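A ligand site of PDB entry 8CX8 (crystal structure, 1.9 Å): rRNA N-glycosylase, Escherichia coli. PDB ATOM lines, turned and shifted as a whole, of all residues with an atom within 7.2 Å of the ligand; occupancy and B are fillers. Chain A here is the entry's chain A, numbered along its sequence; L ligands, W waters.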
ATOM      1  N   GLN A  11      24.141  22.762 -32.363  1.00  0.00           N
ATOM      2  CA  GLN A  11      24.107  21.628 -31.447  1.00  0.00           C
ATOM      3  C   GLN A  11      24.263  22.086 -30.006  1.00  0.00           C
ATOM      4  O   GLN A  11      23.576  21.591 -29.101  1.00  0.00           O
ATOM      5  CB  GLN A  11      25.221  20.647 -31.800  1.00  0.00           C
ATOM      6  CG  GLN A  11      25.153  20.144 -33.223  1.00  0.00           C
ATOM      7  CD  GLN A  11      26.134  19.026 -33.482  1.00  0.00           C
ATOM      8  OE1 GLN A  11      27.117  19.219 -34.197  1.00  0.00           O
ATOM      9  NE2 GLN A  11      25.866  17.864 -32.930  1.00  0.00           N
ATOM     10  N   TYR A  14      21.126  24.062 -28.650  1.00  0.00           N
ATOM     11  CA  TYR A  14      20.016  23.140 -28.391  1.00  0.00           C
ATOM     12  C   TYR A  14      20.203  22.433 -27.052  1.00  0.00           C
ATOM     13  O   TYR A  14      19.297  22.405 -26.216  1.00  0.00           O
ATOM     14  CB  TYR A  14      19.919  22.143 -29.545  1.00  0.00           C
ATOM     15  CG  TYR A  14      18.914  21.012 -29.373  1.00  0.00           C
ATOM     16  CD1 TYR A  14      17.534  21.258 -29.425  1.00  0.00           C
ATOM     17  CD2 TYR A  14      19.349  19.697 -29.188  1.00  0.00           C
ATOM     18  CE1 TYR A  14      16.608  20.201 -29.284  1.00  0.00           C
ATOM     19  CE2 TYR A  14      18.435  18.655 -29.060  1.00  0.00           C
ATOM     20  CZ  TYR A  14      17.065  18.919 -29.106  1.00  0.00           C
ATOM     21  OH  TYR A  14      16.176  17.898 -28.970  1.00  0.00           O
ATOM     22  N   VAL A  15      21.393  21.857 -26.835  1.00  0.00           N
ATOM     23  CA  VAL A  15      21.662  21.152 -25.582  1.00  0.00           C
ATOM     24  C   VAL A  15      21.629  22.111 -24.389  1.00  0.00           C
ATOM     25  O   VAL A  15      21.061  21.779 -23.348  1.00  0.00           O
ATOM     26  CB  VAL A  15      23.007  20.406 -25.661  1.00  0.00           C
ATOM     27  CG1 VAL A  15      23.338  19.800 -24.303  1.00  0.00           C
ATOM     28  CG2 VAL A  15      22.943  19.304 -26.725  1.00  0.00           C
ATOM     29  N   ASN A  19      19.112  22.022 -21.211  1.00  0.00           N
ATOM     30  CA  ASN A  19      19.646  21.965 -19.841  1.00  0.00           C
ATOM     31  C   ASN A  19      19.103  23.100 -18.982  1.00  0.00           C
ATOM     32  O   ASN A  19      18.855  22.908 -17.792  1.00  0.00           O
ATOM     33  CB  ASN A  19      21.171  22.002 -19.844  1.00  0.00           C
ATOM     34  CG  ASN A  19      21.818  20.671 -20.236  1.00  0.00           C
ATOM     35  OD1 ASN A  19      21.196  19.613 -20.110  1.00  0.00           O
ATOM     36  ND2 ASN A  19      23.079  20.728 -20.657  1.00  0.00           N
ATOM     37  N   ARG A  22      15.746  22.087 -17.811  1.00  0.00           N
ATOM     38  CA  ARG A  22      15.836  21.032 -16.800  1.00  0.00           C
ATOM     39  C   ARG A  22      16.280  21.584 -15.449  1.00  0.00           C
ATOM     40  O   ARG A  22      15.724  21.196 -14.404  1.00  0.00           O
ATOM     41  CB  ARG A  22      16.806  19.934 -17.261  1.00  0.00           C
ATOM     42  CG  ARG A  22      16.457  19.265 -18.565  1.00  0.00           C
ATOM     43  CD  ARG A  22      17.516  18.195 -18.871  1.00  0.00           C
ATOM     44  NE  ARG A  22      17.220  17.435 -20.077  1.00  0.00           N
ATOM     45  CZ  ARG A  22      17.999  17.384 -21.153  1.00  0.00           C
ATOM     46  NH1 ARG A  22      19.156  18.045 -21.191  1.00  0.00           N
ATOM     47  NH2 ARG A  22      17.607  16.634 -22.184  1.00  0.00           N
ATOM     48  N   GLN A  34      27.024  12.359 -12.021  1.00  0.00           N
ATOM     49  CA  GLN A  34      28.461  12.339 -12.265  1.00  0.00           C
ATOM     50  C   GLN A  34      28.865  13.684 -12.849  1.00  0.00           C
ATOM     51  O   GLN A  34      28.409  14.045 -13.933  1.00  0.00           O
ATOM     52  CB  GLN A  34      28.853  11.215 -13.223  1.00  0.00           C
ATOM     53  CG  GLN A  34      28.727   9.816 -12.633  1.00  0.00           C
ATOM     54  CD  GLN A  34      29.168   8.742 -13.609  1.00  0.00           C
ATOM     55  OE1 GLN A  34      29.233   8.983 -14.816  1.00  0.00           O
ATOM     56  NE2 GLN A  34      29.476   7.562 -13.086  1.00  0.00           N
ATOM     57  N   THR A  36      28.635  17.337 -13.674  1.00  0.00           N
ATOM     58  CA  THR A  36      27.490  18.234 -13.778  1.00  0.00           C
ATOM     59  C   THR A  36      26.276  17.543 -14.399  1.00  0.00           C
ATOM     60  O   THR A  36      25.283  18.227 -14.698  1.00  0.00           O
ATOM     61  CB  THR A  36      27.850  19.484 -14.581  1.00  0.00           C
ATOM     62  OG1 THR A  36      28.340  19.126 -15.877  1.00  0.00           O
ATOM     63  CG2 THR A  36      28.920  20.291 -13.856  1.00  0.00           C
ATOM     64  N   THR A  37      26.327  16.233 -14.620  1.00  0.00           N
ATOM     65  CA  THR A  37      25.265  15.521 -15.325  1.00  0.00           C
ATOM     66  C   THR A  37      24.495  14.645 -14.337  1.00  0.00           C
ATOM     67  O   THR A  37      25.095  13.925 -13.548  1.00  0.00           O
ATOM     68  CB  THR A  37      25.842  14.647 -16.440  1.00  0.00           C
ATOM     69  OG1 THR A  37      26.496  15.485 -17.398  1.00  0.00           O
ATOM     70  CG2 THR A  37      24.700  13.933 -17.121  1.00  0.00           C
ATOM     71  N   SER A  38      23.166  14.692 -14.421  1.00  0.00           N
ATOM     72  CA  SER A  38      22.368  13.924 -13.481  1.00  0.00           C
ATOM     73  C   SER A  38      21.068  13.479 -14.147  1.00  0.00           C
ATOM     74  O   SER A  38      20.695  13.956 -15.220  1.00  0.00           O
ATOM     75  CB  SER A  38      22.047  14.722 -12.224  1.00  0.00           C
ATOM     76  OG  SER A  38      21.114  15.744 -12.525  1.00  0.00           O
ATOM     77  N   ARG A 173      18.028  11.944 -22.458  1.00  0.00           N
ATOM     78  CA  ARG A 173      19.295  12.377 -23.009  1.00  0.00           C
ATOM     79  C   ARG A 173      19.650  11.581 -24.255  1.00  0.00           C
ATOM     80  O   ARG A 173      20.347  12.097 -25.143  1.00  0.00           O
ATOM     81  CB  ARG A 173      20.374  12.251 -21.928  1.00  0.00           C
ATOM     82  CG  ARG A 173      21.611  13.078 -22.163  1.00  0.00           C
ATOM     83  CD  ARG A 173      22.460  13.228 -20.899  1.00  0.00           C
ATOM     84  NE  ARG A 173      22.022  14.307 -20.027  1.00  0.00           N
ATOM     85  CZ  ARG A 173      21.539  14.159 -18.796  1.00  0.00           C
ATOM     86  NH1 ARG A 173      21.417  12.960 -18.243  1.00  0.00           N
ATOM     87  NH2 ARG A 173      21.195  15.238 -18.112  1.00  0.00           N
ATOM     88  N   GLN A 174      19.184  10.338 -24.360  1.00  0.00           N
ATOM     89  CA  GLN A 174      19.422   9.544 -25.564  1.00  0.00           C
ATOM     90  C   GLN A 174      18.834  10.214 -26.795  1.00  0.00           C
ATOM     91  O   GLN A 174      19.490  10.301 -27.842  1.00  0.00           O
ATOM     92  CB  GLN A 174      18.853   8.127 -25.400  1.00  0.00           C
ATOM     93  CG  GLN A 174      18.867   7.311 -26.690  1.00  0.00           C
ATOM     94  CD  GLN A 174      18.568   5.833 -26.448  1.00  0.00           C
ATOM     95  OE1 GLN A 174      19.165   5.215 -25.580  1.00  0.00           O
ATOM     96  NE2 GLN A 174      17.644   5.271 -27.229  1.00  0.00           N
ATOM     97  N   GLN A 176      17.947  13.463 -27.054  1.00  0.00           N
ATOM     98  CA  GLN A 176      18.689  14.710 -27.235  1.00  0.00           C
ATOM     99  C   GLN A 176      19.967  14.479 -28.041  1.00  0.00           C
ATOM    100  O   GLN A 176      20.279  15.251 -28.961  1.00  0.00           O
ATOM    101  CB  GLN A 176      19.001  15.305 -25.875  1.00  0.00           C
ATOM    102  CG  GLN A 176      20.100  16.341 -25.883  1.00  0.00           C
ATOM    103  CD  GLN A 176      20.542  16.717 -24.490  1.00  0.00           C
ATOM    104  OE1 GLN A 176      19.771  17.298 -23.704  1.00  0.00           O
ATOM    105  NE2 GLN A 176      21.777  16.389 -24.152  1.00  0.00           N
ATOM    106  N   ARG A 177      20.681  13.397 -27.743  1.00  0.00           N
ATOM    107  CA  ARG A 177      21.993  13.168 -28.330  1.00  0.00           C
ATOM    108  C   ARG A 177      21.895  12.715 -29.798  1.00  0.00           C
ATOM    109  O   ARG A 177      22.750  13.087 -30.618  1.00  0.00           O
ATOM    110  CB  ARG A 177      22.744  12.134 -27.494  1.00  0.00           C
ATOM    111  CG  ARG A 177      24.130  11.784 -28.004  1.00  0.00           C
ATOM    112  CD  ARG A 177      24.840  10.791 -27.089  1.00  0.00           C
ATOM    113  NE  ARG A 177      24.050   9.586 -26.850  1.00  0.00           N
ATOM    114  CZ  ARG A 177      23.576   9.229 -25.661  1.00  0.00           C
ATOM    115  NH1 ARG A 177      23.825   9.962 -24.586  1.00  0.00           N
ATOM    116  NH2 ARG A 177      22.855   8.129 -25.533  1.00  0.00           N
ATOM    117  N   GLU A 178      20.885  11.900 -30.134  1.00  0.00           N
ATOM    118  CA  GLU A 178      20.759  11.386 -31.498  1.00  0.00           C
ATOM    119  C   GLU A 178      20.173  12.414 -32.432  1.00  0.00           C
ATOM    120  O   GLU A 178      20.523  12.426 -33.622  1.00  0.00           O
ATOM    121  CB  GLU A 178      19.903  10.122 -31.498  1.00  0.00           C
ATOM    122  CG  GLU A 178      20.552   8.941 -30.780  1.00  0.00           C
ATOM    123  CD  GLU A 178      21.859   8.537 -31.408  1.00  0.00           C
ATOM    124  OE1 GLU A 178      22.014   8.698 -32.650  1.00  0.00           O
ATOM    125  OE2 GLU A 178      22.754   8.071 -30.675  1.00  0.00           O
ATOM    126  N   ARG A 180      20.469  15.855 -31.965  1.00  0.00           N
ATOM    127  CA  ARG A 180      21.173  17.135 -32.044  1.00  0.00           C
ATOM    128  C   ARG A 180      22.129  17.190 -33.223  1.00  0.00           C
ATOM    129  O   ARG A 180      22.390  18.276 -33.748  1.00  0.00           O
ATOM    130  CB  ARG A 180      21.948  17.425 -30.757  1.00  0.00           C
ATOM    131  CG  ARG A 180      23.147  16.534 -30.557  1.00  0.00           C
ATOM    132  CD  ARG A 180      24.152  17.125 -29.580  1.00  0.00           C
ATOM    133  NE  ARG A 180      25.506  16.697 -29.961  1.00  0.00           N
ATOM    134  CZ  ARG A 180      26.179  15.702 -29.409  1.00  0.00           C
ATOM    135  NH1 ARG A 180      25.676  15.029 -28.385  1.00  0.00           N
ATOM    136  NH2 ARG A 180      27.381  15.389 -29.861  1.00  0.00           N
ATOM    137  N   GLN A 181      22.612  16.031 -33.691  1.00  0.00           N
ATOM    138  CA  GLN A 181      23.472  15.955 -34.868  1.00  0.00           C
ATOM    139  C   GLN A 181      22.834  16.588 -36.083  1.00  0.00           C
ATOM    140  O   GLN A 181      23.549  17.054 -36.978  1.00  0.00           O
ATOM    141  CB  GLN A 181      23.777  14.488 -35.205  1.00  0.00           C
ATOM    142  CG  GLN A 181      23.861  13.476 -34.050  1.00  0.00           C
ATOM    143  CD  GLN A 181      25.248  13.376 -33.433  1.00  0.00           C
ATOM    144  OE1 GLN A 181      26.253  13.690 -34.072  1.00  0.00           O
ATOM    145  NE2 GLN A 181      25.293  12.882 -32.198  1.00  0.00           N
ATOM    146  N   ILE A 229      25.649   2.963 -13.981  1.00  0.00           N
ATOM    147  CA  ILE A 229      25.243   4.357 -13.821  1.00  0.00           C
ATOM    148  C   ILE A 229      25.395   5.132 -15.127  1.00  0.00           C
ATOM    149  O   ILE A 229      24.503   5.873 -15.544  1.00  0.00           O
ATOM    150  CB  ILE A 229      26.036   5.035 -12.687  1.00  0.00           C
ATOM    151  CG1 ILE A 229      25.356   4.810 -11.341  1.00  0.00           C
ATOM    152  CG2 ILE A 229      26.181   6.529 -12.947  1.00  0.00           C
ATOM    153  CD1 ILE A 229      24.222   5.763 -11.086  1.00  0.00           C
ATOM    154  N   SER A 230      26.549   4.982 -15.807  1.00  0.00           N
ATOM    155  CA  SER A 230      26.804   5.795 -16.989  1.00  0.00           C
ATOM    156  C   SER A 230      25.765   5.526 -18.076  1.00  0.00           C
ATOM    157  O   SER A 230      25.375   6.442 -18.812  1.00  0.00           O
ATOM    158  CB  SER A 230      28.232   5.587 -17.498  1.00  0.00           C
ATOM    159  OG  SER A 230      28.381   4.378 -18.220  1.00  0.00           O
ATOM    160  N   ALA A 231      25.308   4.273 -18.199  1.00  0.00           N
ATOM    161  CA  ALA A 231      24.238   3.953 -19.143  1.00  0.00           C
ATOM    162  C   ALA A 231      22.940   4.671 -18.775  1.00  0.00           C
ATOM    163  O   ALA A 231      22.189   5.123 -19.648  1.00  0.00           O
ATOM    164  CB  ALA A 231      24.037   2.440 -19.203  1.00  0.00           C
ATOM    165  N   ILE A 232      22.648   4.773 -17.473  1.00  0.00           N
ATOM    166  CA  ILE A 232      21.459   5.512 -17.049  1.00  0.00           C
ATOM    167  C   ILE A 232      21.590   6.983 -17.418  1.00  0.00           C
ATOM    168  O   ILE A 232      20.679   7.570 -18.016  1.00  0.00           O
ATOM    169  CB  ILE A 232      21.212   5.327 -15.540  1.00  0.00           C
ATOM    170  CG1 ILE A 232      21.032   3.848 -15.194  1.00  0.00           C
ATOM    171  CG2 ILE A 232      19.968   6.089 -15.127  1.00  0.00           C
ATOM    172  CD1 ILE A 232      20.971   3.543 -13.714  1.00  0.00           C
ATOM    173  N   LEU A 233      22.713   7.596 -17.034  1.00  0.00           N
ATOM    174  CA  LEU A 233      22.931   9.023 -17.323  1.00  0.00           C
ATOM    175  C   LEU A 233      22.944   9.284 -18.818  1.00  0.00           C
ATOM    176  O   LEU A 233      22.427  10.311 -19.281  1.00  0.00           O
ATOM    177  CB  LEU A 233      24.258   9.486 -16.722  1.00  0.00           C
ATOM    178  CG  LEU A 233      24.318   9.632 -15.204  1.00  0.00           C
ATOM    179  CD1 LEU A 233      25.701  10.135 -14.783  1.00  0.00           C
ATOM    180  CD2 LEU A 233      23.223  10.572 -14.737  1.00  0.00           C
ATOM    181  N   GLY A 234      23.519   8.362 -19.591  1.00  0.00           N
ATOM    182  CA  GLY A 234      23.566   8.488 -21.030  1.00  0.00           C
ATOM    183  C   GLY A 234      22.210   8.484 -21.702  1.00  0.00           C
ATOM    184  O   GLY A 234      22.090   9.002 -22.815  1.00  0.00           O
ATOM    185  N   THR A 235      21.189   7.995 -21.013  1.00  0.00           N
ATOM    186  CA  THR A 235      19.876   7.734 -21.589  1.00  0.00           C
ATOM    187  C   THR A 235      18.792   8.635 -21.019  1.00  0.00           C
ATOM    188  O   THR A 235      18.007   9.204 -21.789  1.00  0.00           O
ATOM    189  CB  THR A 235      19.491   6.252 -21.353  1.00  0.00           C
ATOM    190  OG1 THR A 235      20.551   5.410 -21.815  1.00  0.00           O
ATOM    191  CG2 THR A 235      18.219   5.862 -22.091  1.00  0.00           C
HETATM  192  C1  LIG L   1      26.541  11.379 -21.504  1.00  0.00           C
HETATM  193  C2  LIG L   1      26.975  11.785 -18.820  1.00  0.00           C
HETATM  194  C3  LIG L   1      24.648  15.019 -25.046  1.00  0.00           C
HETATM  195  C4  LIG L   1      25.058  14.843 -23.577  1.00  0.00           C
HETATM  196  C5  LIG L   1      25.088  15.810 -22.577  1.00  0.00           C
HETATM  197  C6  LIG L   1      25.553  15.114 -21.413  1.00  0.00           C
HETATM  198  C7  LIG L   1      25.759  13.788 -21.823  1.00  0.00           C
HETATM  199  C8  LIG L   1      26.275  12.625 -20.956  1.00  0.00           C
HETATM  200  C9  LIG L   1      26.993  10.331 -20.721  1.00  0.00           C
HETATM  201  C10 LIG L   1      26.515  12.837 -19.614  1.00  0.00           C
HETATM  202  C11 LIG L   1      27.218  10.542 -19.370  1.00  0.00           C
HETATM  203  O1  LIG L   1      25.054  14.188 -25.887  1.00  0.00           O
HETATM  204  O2  LIG L   1      23.940  15.981 -25.438  1.00  0.00           O
HETATM  205  O3  LIG L   1      25.455  13.695 -23.085  1.00  0.00           O
HETATM  206 CL1  LIG L   1      27.828   9.220 -18.354  1.00  0.00          CL
HETATM  207  O   HOH W   1      25.327  18.420 -20.484  1.00  0.00           O
HETATM  208  O   HOH W   2      22.524  17.213 -21.355  1.00  0.00           O
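Residues that only touch the ligand: Val 15, Gln 34, Thr 37, Arg 173, Arg 177, Ser 230, Leu 233 and Gly 234.
Hydrophobic or aromatic side chains within 4 Å of the ligand: Val 15 and Leu 233.
Of the 23 residues printed, 10 come within 4 Å of the ligand.
OE1 of Gln 176 is in hydrogen-bond range of NH1 of Arg 22, 2.7 Å away.
NE of Arg 180 sits close to NE2 of Gln 11 (3.2 Å).
The backbone carbonyl oxygen of Gly 234 lies within hydrogen-bond range of the guanidinium group of Arg 177.
The backbone carbonyl oxygen (O) of Arg 177 sits at hydrogen-bond distance from the side-chain amide nitrogen (NE2) of Gln 181, 3.0 Å away.
NH1 of Arg 173 lies within hydrogen-bond range of O of Leu 233 (3.0 Å).
The backbone NH (N) of Arg 173 lies within hydrogen-bond range of the backbone carbonyl oxygen (O) of Thr 235 (2.8 Å).
The guanidinium group (NH2) of Arg 173 lies within hydrogen-bond range of the backbone carbonyl oxygen (O) of Ser 38, at 3.2 Å.
NE2 of Gln 176 sits at hydrogen-bond distance from O2 of the ligand.
The guanidinium group (NH1) of Arg 180 is in salt-bridge range of an oxygen (O1) of the ligand, 2.7 Å away.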
